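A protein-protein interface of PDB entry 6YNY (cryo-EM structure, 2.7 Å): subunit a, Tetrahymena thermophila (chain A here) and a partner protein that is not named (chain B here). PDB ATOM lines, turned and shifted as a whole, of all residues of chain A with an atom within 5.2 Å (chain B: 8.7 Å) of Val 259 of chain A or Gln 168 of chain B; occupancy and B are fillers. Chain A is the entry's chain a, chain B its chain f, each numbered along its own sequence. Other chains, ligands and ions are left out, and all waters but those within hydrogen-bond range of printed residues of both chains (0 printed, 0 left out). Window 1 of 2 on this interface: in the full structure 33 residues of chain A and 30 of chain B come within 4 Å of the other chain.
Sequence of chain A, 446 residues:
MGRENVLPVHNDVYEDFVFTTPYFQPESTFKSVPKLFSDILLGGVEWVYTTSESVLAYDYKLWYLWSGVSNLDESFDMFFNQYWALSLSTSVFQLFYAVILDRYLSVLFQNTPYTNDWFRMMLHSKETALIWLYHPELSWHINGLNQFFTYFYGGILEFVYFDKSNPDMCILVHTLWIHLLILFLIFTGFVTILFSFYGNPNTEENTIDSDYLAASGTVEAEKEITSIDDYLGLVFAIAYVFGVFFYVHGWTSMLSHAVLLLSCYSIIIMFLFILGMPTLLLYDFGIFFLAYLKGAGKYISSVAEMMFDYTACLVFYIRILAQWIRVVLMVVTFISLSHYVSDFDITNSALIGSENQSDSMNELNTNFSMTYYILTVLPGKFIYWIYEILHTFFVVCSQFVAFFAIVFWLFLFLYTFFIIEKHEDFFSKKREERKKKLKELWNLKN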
ATOM      1  N   HIS A 249      12.716  30.203  -0.537  1.00  0.00           N
ATOM      2  CA  HIS A 249      12.984  29.167  -1.522  1.00  0.00           C
ATOM      3  C   HIS A 249      14.170  28.287  -1.157  1.00  0.00           C
ATOM      4  O   HIS A 249      14.550  27.429  -1.957  1.00  0.00           O
ATOM      5  CB  HIS A 249      13.232  29.815  -2.882  1.00  0.00           C
ATOM      6  CG  HIS A 249      14.391  30.757  -2.891  1.00  0.00           C
ATOM      7  ND1 HIS A 249      14.311  32.037  -2.391  1.00  0.00           N
ATOM      8  CD2 HIS A 249      15.660  30.605  -3.333  1.00  0.00           C
ATOM      9  CE1 HIS A 249      15.481  32.633  -2.526  1.00  0.00           C
ATOM     10  NE2 HIS A 249      16.317  31.786  -3.095  1.00  0.00           N
ATOM     11  N   THR A 252      14.047  24.418  -1.419  1.00  0.00           N
ATOM     12  CA  THR A 252      13.827  23.865  -2.749  1.00  0.00           C
ATOM     13  C   THR A 252      15.108  23.843  -3.577  1.00  0.00           C
ATOM     14  O   THR A 252      15.056  23.850  -4.810  1.00  0.00           O
ATOM     15  CB  THR A 252      12.749  24.661  -3.482  1.00  0.00           C
ATOM     16  OG1 THR A 252      13.188  26.011  -3.662  1.00  0.00           O
ATOM     17  CG2 THR A 252      11.452  24.662  -2.696  1.00  0.00           C
ATOM     18  N   SER A 253      16.264  23.809  -2.917  1.00  0.00           N
ATOM     19  CA  SER A 253      17.527  23.926  -3.637  1.00  0.00           C
ATOM     20  C   SER A 253      17.909  22.628  -4.340  1.00  0.00           C
ATOM     21  O   SER A 253      18.438  22.662  -5.455  1.00  0.00           O
ATOM     22  CB  SER A 253      18.633  24.355  -2.676  1.00  0.00           C
ATOM     23  OG  SER A 253      18.293  25.559  -2.020  1.00  0.00           O
ATOM     24  N   SER A 256      15.648  20.515  -7.850  1.00  0.00           N
ATOM     25  CA  SER A 256      15.792  20.719  -9.286  1.00  0.00           C
ATOM     26  C   SER A 256      17.161  21.334  -9.545  1.00  0.00           C
ATOM     27  O   SER A 256      17.947  21.566  -8.623  1.00  0.00           O
ATOM     28  CB  SER A 256      14.675  21.604  -9.834  1.00  0.00           C
ATOM     29  OG  SER A 256      14.685  22.872  -9.209  1.00  0.00           O
ATOM     30  N   HIS A 257      17.436  21.594 -10.821  1.00  0.00           N
ATOM     31  CA  HIS A 257      18.667  22.249 -11.234  1.00  0.00           C
ATOM     32  C   HIS A 257      18.580  23.765 -11.159  1.00  0.00           C
ATOM     33  O   HIS A 257      19.606  24.437 -11.315  1.00  0.00           O
ATOM     34  CB  HIS A 257      19.020  21.828 -12.658  1.00  0.00           C
ATOM     35  CG  HIS A 257      19.274  20.362 -12.804  1.00  0.00           C
ATOM     36  ND1 HIS A 257      18.805  19.630 -13.872  1.00  0.00           N
ATOM     37  CD2 HIS A 257      19.945  19.493 -12.015  1.00  0.00           C
ATOM     38  CE1 HIS A 257      19.177  18.369 -13.733  1.00  0.00           C
ATOM     39  NE2 HIS A 257      19.870  18.260 -12.615  1.00  0.00           N
ATOM     40  N   ALA A 258      17.391  24.313 -10.930  1.00  0.00           N
ATOM     41  CA  ALA A 258      17.188  25.745 -10.787  1.00  0.00           C
ATOM     42  C   ALA A 258      16.605  26.012  -9.410  1.00  0.00           C
ATOM     43  O   ALA A 258      15.503  25.550  -9.098  1.00  0.00           O
ATOM     44  CB  ALA A 258      16.267  26.284 -11.879  1.00  0.00           C
ATOM     45  N   VAL A 259      17.348  26.751  -8.588  1.00  0.00           N
ATOM     46  CA  VAL A 259      16.896  27.039  -7.234  1.00  0.00           C
ATOM     47  C   VAL A 259      15.631  27.883  -7.252  1.00  0.00           C
ATOM     48  O   VAL A 259      14.820  27.818  -6.321  1.00  0.00           O
ATOM     49  CB  VAL A 259      18.025  27.728  -6.445  1.00  0.00           C
ATOM     50  CG1 VAL A 259      17.522  28.204  -5.108  1.00  0.00           C
ATOM     51  CG2 VAL A 259      19.196  26.785  -6.272  1.00  0.00           C
ATOM     52  N   LEU A 260      15.433  28.677  -8.304  1.00  0.00           N
ATOM     53  CA  LEU A 260      14.275  29.552  -8.427  1.00  0.00           C
ATOM     54  C   LEU A 260      13.213  28.987  -9.360  1.00  0.00           C
ATOM     55  O   LEU A 260      12.458  29.748  -9.973  1.00  0.00           O
ATOM     56  CB  LEU A 260      14.709  30.932  -8.910  1.00  0.00           C
ATOM     57  CG  LEU A 260      15.662  31.708  -8.009  1.00  0.00           C
ATOM     58  CD1 LEU A 260      15.966  33.039  -8.635  1.00  0.00           C
ATOM     59  CD2 LEU A 260      15.086  31.900  -6.631  1.00  0.00           C
ATOM     60  N   LEU A 261      13.131  27.664  -9.479  1.00  0.00           N
ATOM     61  CA  LEU A 261      12.133  27.063 -10.355  1.00  0.00           C
ATOM     62  C   LEU A 261      10.724  27.359  -9.863  1.00  0.00           C
ATOM     63  O   LEU A 261       9.885  27.873 -10.610  1.00  0.00           O
ATOM     64  CB  LEU A 261      12.358  25.556 -10.444  1.00  0.00           C
ATOM     65  CG  LEU A 261      11.480  24.830 -11.456  1.00  0.00           C
ATOM     66  CD1 LEU A 261      11.930  25.144 -12.865  1.00  0.00           C
ATOM     67  CD2 LEU A 261      11.504  23.351 -11.197  1.00  0.00           C
ATOM     68  N   LEU A 262      10.446  27.034  -8.602  1.00  0.00           N
ATOM     69  CA  LEU A 262       9.116  27.258  -8.051  1.00  0.00           C
ATOM     70  C   LEU A 262       8.739  28.730  -8.076  1.00  0.00           C
ATOM     71  O   LEU A 262       7.550  29.066  -8.108  1.00  0.00           O
ATOM     72  CB  LEU A 262       9.055  26.711  -6.628  1.00  0.00           C
ATOM     73  CG  LEU A 262       7.779  26.959  -5.831  1.00  0.00           C
ATOM     74  CD1 LEU A 262       6.591  26.300  -6.483  1.00  0.00           C
ATOM     75  CD2 LEU A 262       7.953  26.468  -4.416  1.00  0.00           C
ATOM     76  N   GLY B 115      19.199  27.256   3.443  1.00  0.00           N
ATOM     77  CA  GLY B 115      19.763  27.692   2.178  1.00  0.00           C
ATOM     78  C   GLY B 115      21.272  27.565   2.133  1.00  0.00           C
ATOM     79  O   GLY B 115      21.837  27.078   1.153  1.00  0.00           O
ATOM     80  N   LEU B 118      22.235  23.639   2.261  1.00  0.00           N
ATOM     81  CA  LEU B 118      22.030  22.951   0.994  1.00  0.00           C
ATOM     82  C   LEU B 118      22.937  23.503  -0.095  1.00  0.00           C
ATOM     83  O   LEU B 118      23.335  22.762  -0.999  1.00  0.00           O
ATOM     84  CB  LEU B 118      20.568  23.055   0.573  1.00  0.00           C
ATOM     85  CG  LEU B 118      19.534  22.398   1.488  1.00  0.00           C
ATOM     86  CD1 LEU B 118      18.159  22.535   0.880  1.00  0.00           C
ATOM     87  CD2 LEU B 118      19.851  20.943   1.749  1.00  0.00           C
ATOM     88  N   GLY B 119      23.272  24.790  -0.030  1.00  0.00           N
ATOM     89  CA  GLY B 119      24.198  25.348  -0.996  1.00  0.00           C
ATOM     90  C   GLY B 119      25.605  24.815  -0.817  1.00  0.00           C
ATOM     91  O   GLY B 119      26.318  24.574  -1.794  1.00  0.00           O
ATOM     92  N   LYS B 122      25.550  21.462  -2.268  1.00  0.00           N
ATOM     93  CA  LYS B 122      25.504  21.500  -3.724  1.00  0.00           C
ATOM     94  C   LYS B 122      26.886  21.749  -4.313  1.00  0.00           C
ATOM     95  O   LYS B 122      27.242  21.164  -5.341  1.00  0.00           O
ATOM     96  CB  LYS B 122      24.513  22.566  -4.188  1.00  0.00           C
ATOM     97  CG  LYS B 122      24.242  22.563  -5.680  1.00  0.00           C
ATOM     98  CD  LYS B 122      23.333  23.707  -6.096  1.00  0.00           C
ATOM     99  CE  LYS B 122      21.913  23.531  -5.591  1.00  0.00           C
ATOM    100  NZ  LYS B 122      21.238  22.378  -6.232  1.00  0.00           N
ATOM    101  N   MET B 161      28.508  29.074  -8.919  1.00  0.00           N
ATOM    102  CA  MET B 161      27.428  30.031  -9.083  1.00  0.00           C
ATOM    103  C   MET B 161      27.109  30.677  -7.738  1.00  0.00           C
ATOM    104  O   MET B 161      26.804  29.960  -6.774  1.00  0.00           O
ATOM    105  CB  MET B 161      26.184  29.351  -9.644  1.00  0.00           C
ATOM    106  CG  MET B 161      25.034  30.300  -9.959  1.00  0.00           C
ATOM    107  SD  MET B 161      23.452  29.471 -10.185  1.00  0.00           S
ATOM    108  CE  MET B 161      23.809  28.402 -11.574  1.00  0.00           C
ATOM    109  N   PRO B 162      27.181  32.000  -7.622  1.00  0.00           N
ATOM    110  CA  PRO B 162      26.761  32.640  -6.372  1.00  0.00           C
ATOM    111  C   PRO B 162      25.313  32.302  -6.061  1.00  0.00           C
ATOM    112  O   PRO B 162      24.423  32.464  -6.899  1.00  0.00           O
ATOM    113  CB  PRO B 162      26.957  34.131  -6.653  1.00  0.00           C
ATOM    114  CG  PRO B 162      27.966  34.181  -7.727  1.00  0.00           C
ATOM    115  CD  PRO B 162      27.746  32.973  -8.569  1.00  0.00           C
ATOM    116  N   ALA B 163      25.082  31.817  -4.843  1.00  0.00           N
ATOM    117  CA  ALA B 163      23.760  31.360  -4.428  1.00  0.00           C
ATOM    118  C   ALA B 163      22.876  32.549  -4.051  1.00  0.00           C
ATOM    119  O   ALA B 163      22.390  32.678  -2.929  1.00  0.00           O
ATOM    120  CB  ALA B 163      23.883  30.373  -3.278  1.00  0.00           C
ATOM    121  N   ILE B 164      22.675  33.426  -5.028  1.00  0.00           N
ATOM    122  CA  ILE B 164      21.796  34.577  -4.862  1.00  0.00           C
ATOM    123  C   ILE B 164      20.912  34.668  -6.099  1.00  0.00           C
ATOM    124  O   ILE B 164      21.314  34.213  -7.180  1.00  0.00           O
ATOM    125  CB  ILE B 164      22.588  35.872  -4.625  1.00  0.00           C
ATOM    126  CG1 ILE B 164      23.308  36.330  -5.889  1.00  0.00           C
ATOM    127  CG2 ILE B 164      23.601  35.668  -3.525  1.00  0.00           C
ATOM    128  CD1 ILE B 164      24.086  37.596  -5.687  1.00  0.00           C
ATOM    129  N   PRO B 165      19.715  35.243  -5.993  1.00  0.00           N
ATOM    130  CA  PRO B 165      18.779  35.195  -7.125  1.00  0.00           C
ATOM    131  C   PRO B 165      19.298  35.846  -8.391  1.00  0.00           C
ATOM    132  O   PRO B 165      18.914  35.427  -9.489  1.00  0.00           O
ATOM    133  CB  PRO B 165      17.546  35.924  -6.579  1.00  0.00           C
ATOM    134  CG  PRO B 165      17.659  35.814  -5.109  1.00  0.00           C
ATOM    135  CD  PRO B 165      19.108  35.864  -4.807  1.00  0.00           C
ATOM    136  N   MET B 166      20.157  36.858  -8.281  1.00  0.00           N
ATOM    137  CA  MET B 166      20.651  37.538  -9.472  1.00  0.00           C
ATOM    138  C   MET B 166      21.301  36.553 -10.435  1.00  0.00           C
ATOM    139  O   MET B 166      20.981  36.532 -11.628  1.00  0.00           O
ATOM    140  CB  MET B 166      21.632  38.634  -9.063  1.00  0.00           C
ATOM    141  CG  MET B 166      22.294  39.358 -10.211  1.00  0.00           C
ATOM    142  SD  MET B 166      23.380  40.664  -9.625  1.00  0.00           S
ATOM    143  CE  MET B 166      24.184  41.119 -11.149  1.00  0.00           C
ATOM    144  N   PHE B 167      22.213  35.722  -9.932  1.00  0.00           N
ATOM    145  CA  PHE B 167      22.903  34.761 -10.778  1.00  0.00           C
ATOM    146  C   PHE B 167      22.072  33.517 -11.039  1.00  0.00           C
ATOM    147  O   PHE B 167      22.298  32.834 -12.041  1.00  0.00           O
ATOM    148  CB  PHE B 167      24.230  34.356 -10.139  1.00  0.00           C
ATOM    149  CG  PHE B 167      25.255  35.444 -10.129  1.00  0.00           C
ATOM    150  CD1 PHE B 167      25.274  36.381  -9.119  1.00  0.00           C
ATOM    151  CD2 PHE B 167      26.200  35.528 -11.128  1.00  0.00           C
ATOM    152  CE1 PHE B 167      26.210  37.380  -9.108  1.00  0.00           C
ATOM    153  CE2 PHE B 167      27.143  36.526 -11.120  1.00  0.00           C
ATOM    154  CZ  PHE B 167      27.147  37.454 -10.107  1.00  0.00           C
ATOM    155  N   GLN B 168      21.125  33.206 -10.156  1.00  0.00           N
ATOM    156  CA  GLN B 168      20.276  32.038 -10.341  1.00  0.00           C
ATOM    157  C   GLN B 168      19.237  32.245 -11.432  1.00  0.00           C
ATOM    158  O   GLN B 168      18.649  31.268 -11.904  1.00  0.00           O
ATOM    159  CB  GLN B 168      19.594  31.689  -9.022  1.00  0.00           C
ATOM    160  CG  GLN B 168      20.551  31.237  -7.946  1.00  0.00           C
ATOM    161  CD  GLN B 168      19.951  31.293  -6.563  1.00  0.00           C
ATOM    162  OE1 GLN B 168      18.906  31.904  -6.347  1.00  0.00           O
ATOM    163  NE2 GLN B 168      20.611  30.654  -5.616  1.00  0.00           N
ATOM    164  N   LEU B 169      18.999  33.489 -11.843  1.00  0.00           N
ATOM    165  CA  LEU B 169      18.098  33.768 -12.952  1.00  0.00           C
ATOM    166  C   LEU B 169      18.817  33.792 -14.289  1.00  0.00           C
ATOM    167  O   LEU B 169      18.211  33.474 -15.317  1.00  0.00           O
ATOM    168  CB  LEU B 169      17.402  35.112 -12.737  1.00  0.00           C
ATOM    169  CG  LEU B 169      16.504  35.239 -11.512  1.00  0.00           C
ATOM    170  CD1 LEU B 169      16.097  36.686 -11.320  1.00  0.00           C
ATOM    171  CD2 LEU B 169      15.284  34.358 -11.630  1.00  0.00           C
ATOM    172  N   MET B 170      20.094  34.161 -14.295  1.00  0.00           N
ATOM    173  CA  MET B 170      20.870  34.227 -15.523  1.00  0.00           C
ATOM    174  C   MET B 170      21.502  32.895 -15.884  1.00  0.00           C
ATOM    175  O   MET B 170      21.616  32.572 -17.072  1.00  0.00           O
ATOM    176  CB  MET B 170      21.968  35.284 -15.390  1.00  0.00           C
ATOM    177  CG  MET B 170      21.450  36.686 -15.182  1.00  0.00           C
ATOM    178  SD  MET B 170      22.733  37.938 -15.352  1.00  0.00           S
ATOM    179  CE  MET B 170      23.854  37.439 -14.054  1.00  0.00           C
ATOM    180  N   TYR B 171      21.905  32.116 -14.889  1.00  0.00           N
ATOM    181  CA  TYR B 171      22.608  30.863 -15.090  1.00  0.00           C
ATOM    182  C   TYR B 171      21.777  29.694 -14.585  1.00  0.00           C
ATOM    183  O   TYR B 171      20.901  29.847 -13.731  1.00  0.00           O
ATOM    184  CB  TYR B 171      23.954  30.861 -14.358  1.00  0.00           C
ATOM    185  CG  TYR B 171      24.901  31.974 -14.721  1.00  0.00           C
ATOM    186  CD1 TYR B 171      25.893  32.369 -13.840  1.00  0.00           C
ATOM    187  CD2 TYR B 171      24.818  32.620 -15.940  1.00  0.00           C
ATOM    188  CE1 TYR B 171      26.769  33.376 -14.160  1.00  0.00           C
ATOM    189  CE2 TYR B 171      25.689  33.628 -16.267  1.00  0.00           C
ATOM    190  CZ  TYR B 171      26.663  34.002 -15.376  1.00  0.00           C
ATOM    191  OH  TYR B 171      27.536  35.009 -15.703  1.00  0.00           O
ATOM    192  N   TYR B 172      22.069  28.516 -15.127  1.00  0.00           N
ATOM    193  CA  TYR B 172      21.589  27.273 -14.546  1.00  0.00           C
ATOM    194  C   TYR B 172      22.533  26.157 -14.958  1.00  0.00           C
ATOM    195  O   TYR B 172      23.089  26.169 -16.059  1.00  0.00           O
ATOM    196  CB  TYR B 172      20.146  26.952 -14.951  1.00  0.00           C
ATOM    197  CG  TYR B 172      19.918  26.646 -16.406  1.00  0.00           C
ATOM    198  CD1 TYR B 172      19.948  25.344 -16.873  1.00  0.00           C
ATOM    199  CD2 TYR B 172      19.636  27.653 -17.309  1.00  0.00           C
ATOM    200  CE1 TYR B 172      19.725  25.058 -18.197  1.00  0.00           C
ATOM    201  CE2 TYR B 172      19.412  27.377 -18.631  1.00  0.00           C
ATOM    202  CZ  TYR B 172      19.456  26.080 -19.072  1.00  0.00           C
ATOM    203  OH  TYR B 172      19.230  25.808 -20.395  1.00  0.00           O
ATOM    204  N   GLU B 173      22.716  25.204 -14.051  1.00  0.00           N
ATOM    205  CA  GLU B 173      23.684  24.141 -14.262  1.00  0.00           C
ATOM    206  C   GLU B 173      23.284  23.271 -15.444  1.00  0.00           C
ATOM    207  O   GLU B 173      22.103  23.106 -15.758  1.00  0.00           O
ATOM    208  CB  GLU B 173      23.811  23.281 -13.006  1.00  0.00           C
ATOM    209  CG  GLU B 173      24.181  24.054 -11.758  1.00  0.00           C
ATOM    210  CD  GLU B 173      25.538  24.719 -11.856  1.00  0.00           C
ATOM    211  OE1 GLU B 173      26.322  24.348 -12.752  1.00  0.00           O
ATOM    212  OE2 GLU B 173      25.819  25.616 -11.037  1.00  0.00           O
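Among the printed residues, merely in contact across the chains: Ser 253 of chain A with Leu 118 of chain B (3.999 Å), Val 259 of chain A with Gln 168 of chain B (3.98 Å), Leu 260 of chain A with Pro 165 of chain B (3.9 Å), Leu 260 of chain A with Gln 168 of chain B (3.7 Å) and Leu 260 of chain A with Leu 169 of chain B (3.3 Å).
Of the printed residues of chain B, Ser 253 of chain A touches Leu 118 (3.999 Å) and Lys 122 (2.9 Å).
No residue of chain B comes within 4 Å of Ala 258 of chain A.
Val 259 of chain A touches just one residue of chain B: Gln 168 (3.98 Å).
Leu 260 of chain A touches just these residues of chain B: Pro 165 (3.9 Å), Gln 168 (3.7 Å) and Leu 169 (3.3 Å).
Of the printed residues of chain A, Pro 165 of chain B touches Leu 260.
NZ of Lys 122 of chain B lies within hydrogen-bond range of O of Ser 253 of chain A, 2.9 Å away.
OE1 of Gln 168 of chain B sits close to O of Ile 164 of chain B (3.4 Å).
Of the 10 printed residues of chain A, 3 touch a printed residue of chain B.
Hydrophobic or aromatic side chains of chain A within 4 Å of the printed part of chain B: Val 259 and Leu 260.
Along chain A the printed residues that touch a printed residue of chain B span positions 253 to 260.
Of the 17 printed residues of chain B, 5 touch a printed residue of chain A.
Along chain B the printed residues that touch a printed residue of chain A span positions 118 to 169.
Among the printed residues, 6 pairs touch across the chains.
Among the printed residues, no Asp or Glu carboxylate lies within 4 Å of a Lys or Arg side-chain nitrogen of the other chain.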
